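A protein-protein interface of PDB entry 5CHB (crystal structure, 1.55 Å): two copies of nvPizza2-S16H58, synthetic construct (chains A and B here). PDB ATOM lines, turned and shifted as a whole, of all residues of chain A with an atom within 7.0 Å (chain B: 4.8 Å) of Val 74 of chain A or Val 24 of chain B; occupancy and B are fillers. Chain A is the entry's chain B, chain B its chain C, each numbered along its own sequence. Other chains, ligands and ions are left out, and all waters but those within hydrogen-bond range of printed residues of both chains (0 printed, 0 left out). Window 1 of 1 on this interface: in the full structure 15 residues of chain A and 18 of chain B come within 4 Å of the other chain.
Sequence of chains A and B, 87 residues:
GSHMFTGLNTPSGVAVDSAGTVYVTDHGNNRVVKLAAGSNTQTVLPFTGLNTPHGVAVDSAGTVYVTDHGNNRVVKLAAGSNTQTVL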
ATOM      1  N   TYR A  65      25.319 -13.453   5.975  1.00  0.00           N
ATOM      2  CA  TYR A  65      24.249 -14.341   5.390  1.00  0.00           C
ATOM      3  C   TYR A  65      24.873 -14.949   4.138  1.00  0.00           C
ATOM      4  O   TYR A  65      25.380 -14.235   3.294  1.00  0.00           O
ATOM      5  CB  TYR A  65      23.066 -13.541   5.017  1.00  0.00           C
ATOM      6  CG  TYR A  65      22.450 -12.770   6.177  1.00  0.00           C
ATOM      7  CD1 TYR A  65      23.027 -11.574   6.629  1.00  0.00           C
ATOM      8  CD2 TYR A  65      21.351 -13.246   6.835  1.00  0.00           C
ATOM      9  CE1 TYR A  65      22.446 -10.892   7.677  1.00  0.00           C
ATOM     10  CE2 TYR A  65      20.772 -12.529   7.871  1.00  0.00           C
ATOM     11  CZ  TYR A  65      21.354 -11.363   8.280  1.00  0.00           C
ATOM     12  OH  TYR A  65      20.823 -10.579   9.355  1.00  0.00           O
ATOM     13  N   VAL A  66      24.724 -16.260   4.000  1.00  0.00           N
ATOM     14  CA  VAL A  66      25.345 -16.948   2.873  1.00  0.00           C
ATOM     15  C   VAL A  66      24.324 -17.874   2.258  1.00  0.00           C
ATOM     16  O   VAL A  66      23.626 -18.619   2.999  1.00  0.00           O
ATOM     17  CB  VAL A  66      26.571 -17.781   3.326  1.00  0.00           C
ATOM     18  CG1 VAL A  66      27.069 -18.703   2.253  1.00  0.00           C
ATOM     19  CG2 VAL A  66      27.703 -16.832   3.689  1.00  0.00           C
ATOM     20  N   THR A  67      24.244 -17.869   0.919  1.00  0.00           N
ATOM     21  CA  THR A  67      23.429 -18.912   0.252  1.00  0.00           C
ATOM     22  C   THR A  67      24.248 -20.208   0.133  1.00  0.00           C
ATOM     23  O   THR A  67      25.321 -20.267  -0.449  1.00  0.00           O
ATOM     24  CB  THR A  67      22.933 -18.439  -1.074  1.00  0.00           C
ATOM     25  OG1 THR A  67      24.068 -18.073  -1.877  1.00  0.00           O
ATOM     26  CG2 THR A  67      22.002 -17.295  -0.945  1.00  0.00           C
ATOM     27  N   ASP A  68      23.694 -21.278   0.681  1.00  0.00           N
ATOM     28  CA  ASP A  68      24.332 -22.581   0.731  1.00  0.00           C
ATOM     29  C   ASP A  68      23.671 -23.365  -0.437  1.00  0.00           C
ATOM     30  O   ASP A  68      22.646 -23.971  -0.302  1.00  0.00           O
ATOM     31  CB  ASP A  68      24.110 -23.246   2.054  1.00  0.00           C
ATOM     32  CG  ASP A  68      24.944 -24.458   2.232  1.00  0.00           C
ATOM     33  OD1 ASP A  68      25.656 -24.831   1.292  1.00  0.00           O
ATOM     34  OD2 ASP A  68      24.843 -25.079   3.341  1.00  0.00           O
ATOM     35  N   ASN A  71      22.679 -27.021  -0.480  1.00  0.00           N
ATOM     36  CA  ASN A  71      21.788 -27.453   0.589  1.00  0.00           C
ATOM     37  C   ASN A  71      20.483 -26.739   0.583  1.00  0.00           C
ATOM     38  O   ASN A  71      19.654 -26.821   1.529  1.00  0.00           O
ATOM     39  CB  ASN A  71      22.471 -27.266   1.951  1.00  0.00           C
ATOM     40  CG  ASN A  71      23.543 -28.294   2.183  1.00  0.00           C
ATOM     41  OD1 ASN A  71      23.381 -29.465   1.770  1.00  0.00           O
ATOM     42  ND2 ASN A  71      24.625 -27.908   2.809  1.00  0.00           N
ATOM     43  N   ASN A  72      20.269 -25.960  -0.479  1.00  0.00           N
ATOM     44  CA  ASN A  72      18.991 -25.288  -0.599  1.00  0.00           C
ATOM     45  C   ASN A  72      18.545 -24.505   0.584  1.00  0.00           C
ATOM     46  O   ASN A  72      17.403 -24.554   1.033  1.00  0.00           O
ATOM     47  CB  ASN A  72      17.922 -26.314  -1.076  1.00  0.00           C
ATOM     48  CG  ASN A  72      18.407 -27.142  -2.222  1.00  0.00           C
ATOM     49  OD1 ASN A  72      18.696 -26.631  -3.287  1.00  0.00           O
ATOM     50  ND2 ASN A  72      18.530 -28.422  -2.015  1.00  0.00           N
ATOM     51  N   ARG A  73      19.486 -23.699   1.140  1.00  0.00           N
ATOM     52  CA  ARG A  73      19.258 -23.041   2.373  1.00  0.00           C
ATOM     53  C   ARG A  73      20.114 -21.770   2.472  1.00  0.00           C
ATOM     54  O   ARG A  73      21.091 -21.605   1.697  1.00  0.00           O
ATOM     55  CB  ARG A  73      19.535 -23.888   3.576  1.00  0.00           C
ATOM     56  CG  ARG A  73      20.968 -24.237   3.780  1.00  0.00           C
ATOM     57  CD  ARG A  73      21.225 -25.208   4.924  1.00  0.00           C
ATOM     58  NE  ARG A  73      22.645 -25.467   5.053  1.00  0.00           N
ATOM     59  CZ  ARG A  73      23.252 -26.022   6.094  1.00  0.00           C
ATOM     60  NH1 ARG A  73      22.537 -26.401   7.129  1.00  0.00           N
ATOM     61  NH2 ARG A  73      24.566 -26.127   6.137  1.00  0.00           N
ATOM     62  N   VAL A  74      19.742 -20.905   3.398  1.00  0.00           N
ATOM     63  CA  VAL A  74      20.530 -19.725   3.689  1.00  0.00           C
ATOM     64  C   VAL A  74      21.008 -19.844   5.115  1.00  0.00           C
ATOM     65  O   VAL A  74      20.173 -20.236   5.993  1.00  0.00           O
ATOM     66  CB  VAL A  74      19.692 -18.468   3.488  1.00  0.00           C
ATOM     67  CG1 VAL A  74      20.416 -17.212   3.829  1.00  0.00           C
ATOM     68  CG2 VAL A  74      19.157 -18.466   2.097  1.00  0.00           C
ATOM     69  N   VAL A  75      22.284 -19.644   5.361  1.00  0.00           N
ATOM     70  CA  VAL A  75      22.871 -19.735   6.713  1.00  0.00           C
ATOM     71  C   VAL A  75      23.334 -18.351   7.173  1.00  0.00           C
ATOM     72  O   VAL A  75      23.718 -17.485   6.373  1.00  0.00           O
ATOM     73  CB  VAL A  75      23.973 -20.718   6.800  1.00  0.00           C
ATOM     74  CG1 VAL A  75      23.365 -22.119   6.546  1.00  0.00           C
ATOM     75  CG2 VAL A  75      25.073 -20.440   5.851  1.00  0.00           C
ATOM     76  N   LYS A  76      23.234 -18.088   8.479  1.00  0.00           N
ATOM     77  CA  LYS A  76      23.726 -16.841   9.003  1.00  0.00           C
ATOM     78  C   LYS A  76      24.638 -17.036  10.185  1.00  0.00           C
ATOM     79  O   LYS A  76      24.533 -18.018  10.947  1.00  0.00           O
ATOM     80  CB  LYS A  76      22.614 -15.858   9.264  1.00  0.00           C
ATOM     81  CG  LYS A  76      21.821 -16.091  10.453  1.00  0.00           C
ATOM     82  CD  LYS A  76      20.957 -14.872  10.775  1.00  0.00           C
ATOM     83  CE  LYS A  76      19.850 -15.286  11.699  1.00  0.00           C
ATOM     84  NZ  LYS A  76      19.247 -14.061  12.250  1.00  0.00           N
ATOM     85  N   THR A  85      23.098 -20.248  12.217  1.00  0.00           N
ATOM     86  CA  THR A  85      21.632 -20.455  12.239  1.00  0.00           C
ATOM     87  C   THR A  85      21.195 -20.682  10.783  1.00  0.00           C
ATOM     88  O   THR A  85      21.704 -20.035   9.890  1.00  0.00           O
ATOM     89  CB  THR A  85      20.855 -19.208  12.781  1.00  0.00           C
ATOM     90  OG1 THR A  85      21.116 -19.013  14.185  1.00  0.00           O
ATOM     91  CG2 THR A  85      19.311 -19.306  12.548  1.00  0.00           C
ATOM     92  N   VAL A  86      20.263 -21.573  10.551  1.00  0.00           N
ATOM     93  CA  VAL A  86      19.674 -21.735   9.234  1.00  0.00           C
ATOM     94  C   VAL A  86      18.400 -20.901   9.098  1.00  0.00           C
ATOM     95  O   VAL A  86      17.526 -20.996   9.969  1.00  0.00           O
ATOM     96  CB  VAL A  86      19.338 -23.187   8.990  1.00  0.00           C
ATOM     97  CG1 VAL A  86      18.704 -23.371   7.608  1.00  0.00           C
ATOM     98  CG2 VAL A  86      20.569 -24.024   9.135  1.00  0.00           C
ATOM     99  N   LEU A  87      18.234 -20.152   8.019  1.00  0.00           N
ATOM    100  CA  LEU A  87      17.020 -19.320   7.842  1.00  0.00           C
ATOM    101  C   LEU A  87      15.797 -20.043   7.380  1.00  0.00           C
ATOM    102  O   LEU A  87      15.818 -21.029   6.636  1.00  0.00           O
ATOM    103  CB  LEU A  87      17.222 -18.089   6.976  1.00  0.00           C
ATOM    104  CG  LEU A  87      17.908 -16.958   7.706  1.00  0.00           C
ATOM    105  CD1 LEU A  87      19.304 -17.284   8.034  1.00  0.00           C
ATOM    106  CD2 LEU A  87      17.964 -15.749   6.822  1.00  0.00           C
ATOM    107  OXT LEU A  87      14.709 -19.550   7.779  1.00  0.00           O
ATOM    108  N   PHE B   5      12.550 -20.276   5.692  1.00  0.00           N
ATOM    109  CA  PHE B   5      12.312 -20.279   4.243  1.00  0.00           C
ATOM    110  C   PHE B   5      11.778 -21.678   3.868  1.00  0.00           C
ATOM    111  O   PHE B   5      12.122 -22.664   4.518  1.00  0.00           O
ATOM    112  CB  PHE B   5      13.557 -20.032   3.382  1.00  0.00           C
ATOM    113  CG  PHE B   5      14.009 -18.589   3.256  1.00  0.00           C
ATOM    114  CD1 PHE B   5      13.271 -17.628   2.567  1.00  0.00           C
ATOM    115  CD2 PHE B   5      15.248 -18.212   3.774  1.00  0.00           C
ATOM    116  CE1 PHE B   5      13.733 -16.355   2.413  1.00  0.00           C
ATOM    117  CE2 PHE B   5      15.715 -16.922   3.560  1.00  0.00           C
ATOM    118  CZ  PHE B   5      14.932 -15.987   2.971  1.00  0.00           C
ATOM    119  N   LEU B   8      13.131 -23.675  -1.090  1.00  0.00           N
ATOM    120  CA  LEU B   8      14.267 -23.141  -1.849  1.00  0.00           C
ATOM    121  C   LEU B   8      14.918 -24.197  -2.750  1.00  0.00           C
ATOM    122  O   LEU B   8      14.835 -25.402  -2.458  1.00  0.00           O
ATOM    123  CB  LEU B   8      15.309 -22.535  -0.924  1.00  0.00           C
ATOM    124  CG  LEU B   8      14.887 -21.311  -0.119  1.00  0.00           C
ATOM    125  CD1 LEU B   8      16.128 -20.725   0.554  1.00  0.00           C
ATOM    126  CD2 LEU B   8      14.222 -20.208  -0.911  1.00  0.00           C
ATOM    127  N   PRO B  11      19.515 -21.663  -4.094  1.00  0.00           N
ATOM    128  CA  PRO B  11      19.633 -20.213  -3.940  1.00  0.00           C
ATOM    129  C   PRO B  11      21.010 -19.672  -4.306  1.00  0.00           C
ATOM    130  O   PRO B  11      22.039 -20.302  -4.084  1.00  0.00           O
ATOM    131  CB  PRO B  11      19.276 -20.039  -2.466  1.00  0.00           C
ATOM    132  CG  PRO B  11      19.762 -21.307  -1.792  1.00  0.00           C
ATOM    133  CD  PRO B  11      19.417 -22.340  -2.814  1.00  0.00           C
ATOM    134  N   GLY B  13      21.791 -15.535  -5.073  1.00  0.00           N
ATOM    135  CA  GLY B  13      22.009 -14.155  -4.543  1.00  0.00           C
ATOM    136  C   GLY B  13      21.361 -13.981  -3.204  1.00  0.00           C
ATOM    137  O   GLY B  13      20.328 -14.602  -2.895  1.00  0.00           O
ATOM    138  N   VAL B  14      21.890 -13.078  -2.352  1.00  0.00           N
ATOM    139  CA  VAL B  14      21.305 -12.754  -1.056  1.00  0.00           C
ATOM    140  C   VAL B  14      21.593 -11.277  -0.762  1.00  0.00           C
ATOM    141  O   VAL B  14      22.672 -10.747  -1.172  1.00  0.00           O
ATOM    142  CB  VAL B  14      21.794 -13.688   0.081  1.00  0.00           C
ATOM    143  CG1 VAL B  14      23.321 -13.698   0.194  1.00  0.00           C
ATOM    144  CG2 VAL B  14      21.096 -13.477   1.396  1.00  0.00           C
ATOM    145  N   VAL B  22      15.678 -10.380   4.799  1.00  0.00           N
ATOM    146  CA  VAL B  22      16.616 -11.070   3.946  1.00  0.00           C
ATOM    147  C   VAL B  22      15.942 -11.377   2.609  1.00  0.00           C
ATOM    148  O   VAL B  22      14.838 -11.902   2.604  1.00  0.00           O
ATOM    149  CB  VAL B  22      17.110 -12.339   4.604  1.00  0.00           C
ATOM    150  CG1 VAL B  22      18.062 -13.098   3.731  1.00  0.00           C
ATOM    151  CG2 VAL B  22      17.814 -11.941   5.954  1.00  0.00           C
ATOM    152  N   TYR B  23      16.615 -11.106   1.519  1.00  0.00           N
ATOM    153  CA  TYR B  23      16.160 -11.242   0.145  1.00  0.00           C
ATOM    154  C   TYR B  23      17.073 -12.291  -0.504  1.00  0.00           C
ATOM    155  O   TYR B  23      18.259 -12.248  -0.410  1.00  0.00           O
ATOM    156  CB  TYR B  23      16.272  -9.938  -0.593  1.00  0.00           C
ATOM    157  CG  TYR B  23      15.517  -8.795   0.000  1.00  0.00           C
ATOM    158  CD1 TYR B  23      16.080  -8.105   1.109  1.00  0.00           C
ATOM    159  CD2 TYR B  23      14.358  -8.356  -0.544  1.00  0.00           C
ATOM    160  CE1 TYR B  23      15.389  -7.072   1.667  1.00  0.00           C
ATOM    161  CE2 TYR B  23      13.636  -7.343   0.050  1.00  0.00           C
ATOM    162  CZ  TYR B  23      14.195  -6.718   1.164  1.00  0.00           C
ATOM    163  OH  TYR B  23      13.559  -5.621   1.730  1.00  0.00           O
ATOM    164  N   VAL B  24      16.436 -13.260  -1.177  1.00  0.00           N
ATOM    165  CA  VAL B  24      17.231 -14.348  -1.795  1.00  0.00           C
ATOM    166  C   VAL B  24      16.738 -14.599  -3.237  1.00  0.00           C
ATOM    167  O   VAL B  24      15.552 -14.681  -3.435  1.00  0.00           O
ATOM    168  CB  VAL B  24      17.059 -15.646  -1.004  1.00  0.00           C
ATOM    169  CG1 VAL B  24      17.720 -16.822  -1.697  1.00  0.00           C
ATOM    170  CG2 VAL B  24      17.587 -15.466   0.405  1.00  0.00           C
ATOM    171  N   THR B  25      17.637 -14.729  -4.207  1.00  0.00           N
ATOM    172  CA  THR B  25      17.246 -15.253  -5.530  1.00  0.00           C
ATOM    173  C   THR B  25      17.252 -16.768  -5.446  1.00  0.00           C
ATOM    174  O   THR B  25      18.272 -17.425  -5.259  1.00  0.00           O
ATOM    175  CB  THR B  25      18.066 -14.682  -6.720  1.00  0.00           C
ATOM    176  OG1 THR B  25      19.417 -15.138  -6.674  1.00  0.00           O
ATOM    177  CG2 THR B  25      17.999 -13.214  -6.728  1.00  0.00           C
ATOM    178  N   ASP B  26      16.039 -17.320  -5.584  1.00  0.00           N
ATOM    179  CA  ASP B  26      15.829 -18.722  -5.521  1.00  0.00           C
ATOM    180  C   ASP B  26      15.975 -19.243  -6.914  1.00  0.00           C
ATOM    181  O   ASP B  26      15.047 -19.455  -7.690  1.00  0.00           O
ATOM    182  CB  ASP B  26      14.440 -18.974  -4.940  1.00  0.00           C
ATOM    183  CG  ASP B  26      14.236 -20.398  -4.579  1.00  0.00           C
ATOM    184  OD1 ASP B  26      15.253 -21.091  -4.389  1.00  0.00           O
ATOM    185  OD2 ASP B  26      13.042 -20.824  -4.354  1.00  0.00           O
ATOM    186  N   ARG B  31      12.459 -17.388  -9.032  1.00  0.00           N
ATOM    187  CA  ARG B  31      11.776 -16.423  -8.206  1.00  0.00           C
ATOM    188  C   ARG B  31      12.715 -15.750  -7.167  1.00  0.00           C
ATOM    189  O   ARG B  31      13.796 -16.274  -6.906  1.00  0.00           O
ATOM    190  CB  ARG B  31      10.645 -17.132  -7.430  1.00  0.00           C
ATOM    191  CG  ARG B  31      11.099 -18.079  -6.388  1.00  0.00           C
ATOM    192  CD  ARG B  31       9.980 -18.802  -5.641  1.00  0.00           C
ATOM    193  NE  ARG B  31      10.528 -19.675  -4.674  1.00  0.00           N
ATOM    194  CZ  ARG B  31       9.843 -20.272  -3.705  1.00  0.00           C
ATOM    195  NH1 ARG B  31       8.556 -20.057  -3.615  1.00  0.00           N
ATOM    196  NH2 ARG B  31      10.432 -21.034  -2.859  1.00  0.00           N
ATOM    197  N   VAL B  32      12.259 -14.630  -6.623  1.00  0.00           N
ATOM    198  CA  VAL B  32      12.947 -13.903  -5.572  1.00  0.00           C
ATOM    199  C   VAL B  32      12.063 -13.939  -4.314  1.00  0.00           C
ATOM    200  O   VAL B  32      10.887 -13.630  -4.404  1.00  0.00           O
ATOM    201  CB  VAL B  32      13.295 -12.500  -6.036  1.00  0.00           C
ATOM    202  CG1 VAL B  32      14.061 -11.752  -4.974  1.00  0.00           C
ATOM    203  CG2 VAL B  32      14.106 -12.576  -7.341  1.00  0.00           C
ATOM    204  N   VAL B  33      12.617 -14.405  -3.212  1.00  0.00           N
ATOM    205  CA  VAL B  33      11.858 -14.510  -1.970  1.00  0.00           C
ATOM    206  C   VAL B  33      12.480 -13.610  -0.901  1.00  0.00           C
ATOM    207  O   VAL B  33      13.644 -13.213  -1.036  1.00  0.00           O
ATOM    208  CB  VAL B  33      11.812 -15.954  -1.476  1.00  0.00           C
ATOM    209  CG1 VAL B  33      11.108 -16.813  -2.527  1.00  0.00           C
ATOM    210  CG2 VAL B  33      13.126 -16.541  -1.092  1.00  0.00           C
ATOM    211  N   VAL B  56      20.953 -10.281  -6.325  1.00  0.00           N
ATOM    212  CA  VAL B  56      20.004  -9.311  -5.735  1.00  0.00           C
ATOM    213  C   VAL B  56      20.755  -8.284  -4.816  1.00  0.00           C
ATOM    214  O   VAL B  56      21.747  -8.586  -4.157  1.00  0.00           O
ATOM    215  CB  VAL B  56      18.880 -10.058  -4.941  1.00  0.00           C
ATOM    216  CG1 VAL B  56      19.400 -10.905  -3.837  1.00  0.00           C
ATOM    217  CG2 VAL B  56      17.817  -9.083  -4.450  1.00  0.00           C
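The backbone NH of Phe 5 of chain B is in hydrogen-bond range of the chain-end carboxylate of Leu 87 of chain A, at 3.1 Å.
The side-chain carboxylate (OD2) of Asp 68 of chain A is in salt-bridge range of the guanidinium group (NE) of Arg 73 of chain A, 2.8 Å away.
N of Val 24 of chain B is in hydrogen-bond range of O of Val 33 of chain B (2.8 Å).
OG1 of Thr 25 of chain B lies within hydrogen-bond range of N of Gly 13 of chain B (2.9 Å).
The backbone carbonyl oxygen (O) of Val 74 of chain A sits at hydrogen-bond distance from the backbone NH (N) of Leu 87 of chain A (2.8 Å).
Among the printed residues, merely in contact across the chains: Tyr 65 of chain A with Val 14 of chain B (3.8 Å), Tyr 65 of chain A with Val 22 of chain B (3.6 Å), Thr 67 of chain A with Pro 11 of chain B (3.7 Å), Thr 67 of chain A with Gly 13 of chain B (3.7 Å), Thr 67 of chain A with Val 14 of chain B (3.8 Å), Asn 72 of chain A with Leu 8 of chain B (3.5 Å), Asn 72 of chain A with Pro 11 of chain B (3.7 Å), Arg 73 of chain A with Pro 11 of chain B (3.7 Å), Val 74 of chain A with Val 24 of chain B (3.8 Å) and Leu 87 of chain A with Val 22 of chain B (3.9 Å).
Of the printed residues of chain B, Arg 73 of chain A touches Pro 11 (3.7 Å).
Of chain B, only Val 24 (3.8 Å) comes within 4 Å of Val 74 of chain A.
Thr 85 of chain A touches none of the printed residues of chain B.
Printed residues of chain B within 4 Å of Leu 87 of chain A: Phe 5 (3.1 Å) and Val 22 (3.9 Å).
Printed residues of chain A within 4 Å of Phe 5 of chain B: Leu 87 (3.1 Å).
Printed residues of chain A within 4 Å of Leu 8 of chain B: Asn 72 (3.5 Å).
Of the printed residues of chain A, Gly 13 of chain B touches Thr 67.
Of chain A, only Val 74 comes within 4 Å of Val 24 of chain B.
The nearest residue of chain A that does not touch Val 24 of chain B is Thr 67 of chain A (4.4 Å).
Hydrophobic or aromatic side chains of chain B that line the printed part of chain A: Phe 5, Leu 8, Pro 11, Val 14, Val 22 and Val 24.
Printed residues of chain A that touch a printed residue of chain B: Tyr 65, Thr 67, Asn 72, Arg 73, Val 74 and Leu 87.
Hydrophobic or aromatic side chains of chain A within 4 Å of the printed part of chain B: Tyr 65, Val 74 and Leu 87.
Among the printed residues, 11 pairs touch across the chains.
Among the printed residues, no Asp or Glu carboxylate lies within 4 Å of a Lys or Arg side-chain nitrogen of the other chain.
No position is printed for both chains.
Of the 11 pairs that touch across the chains among the printed residues, none has its exchanged pair printed and touching as well.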
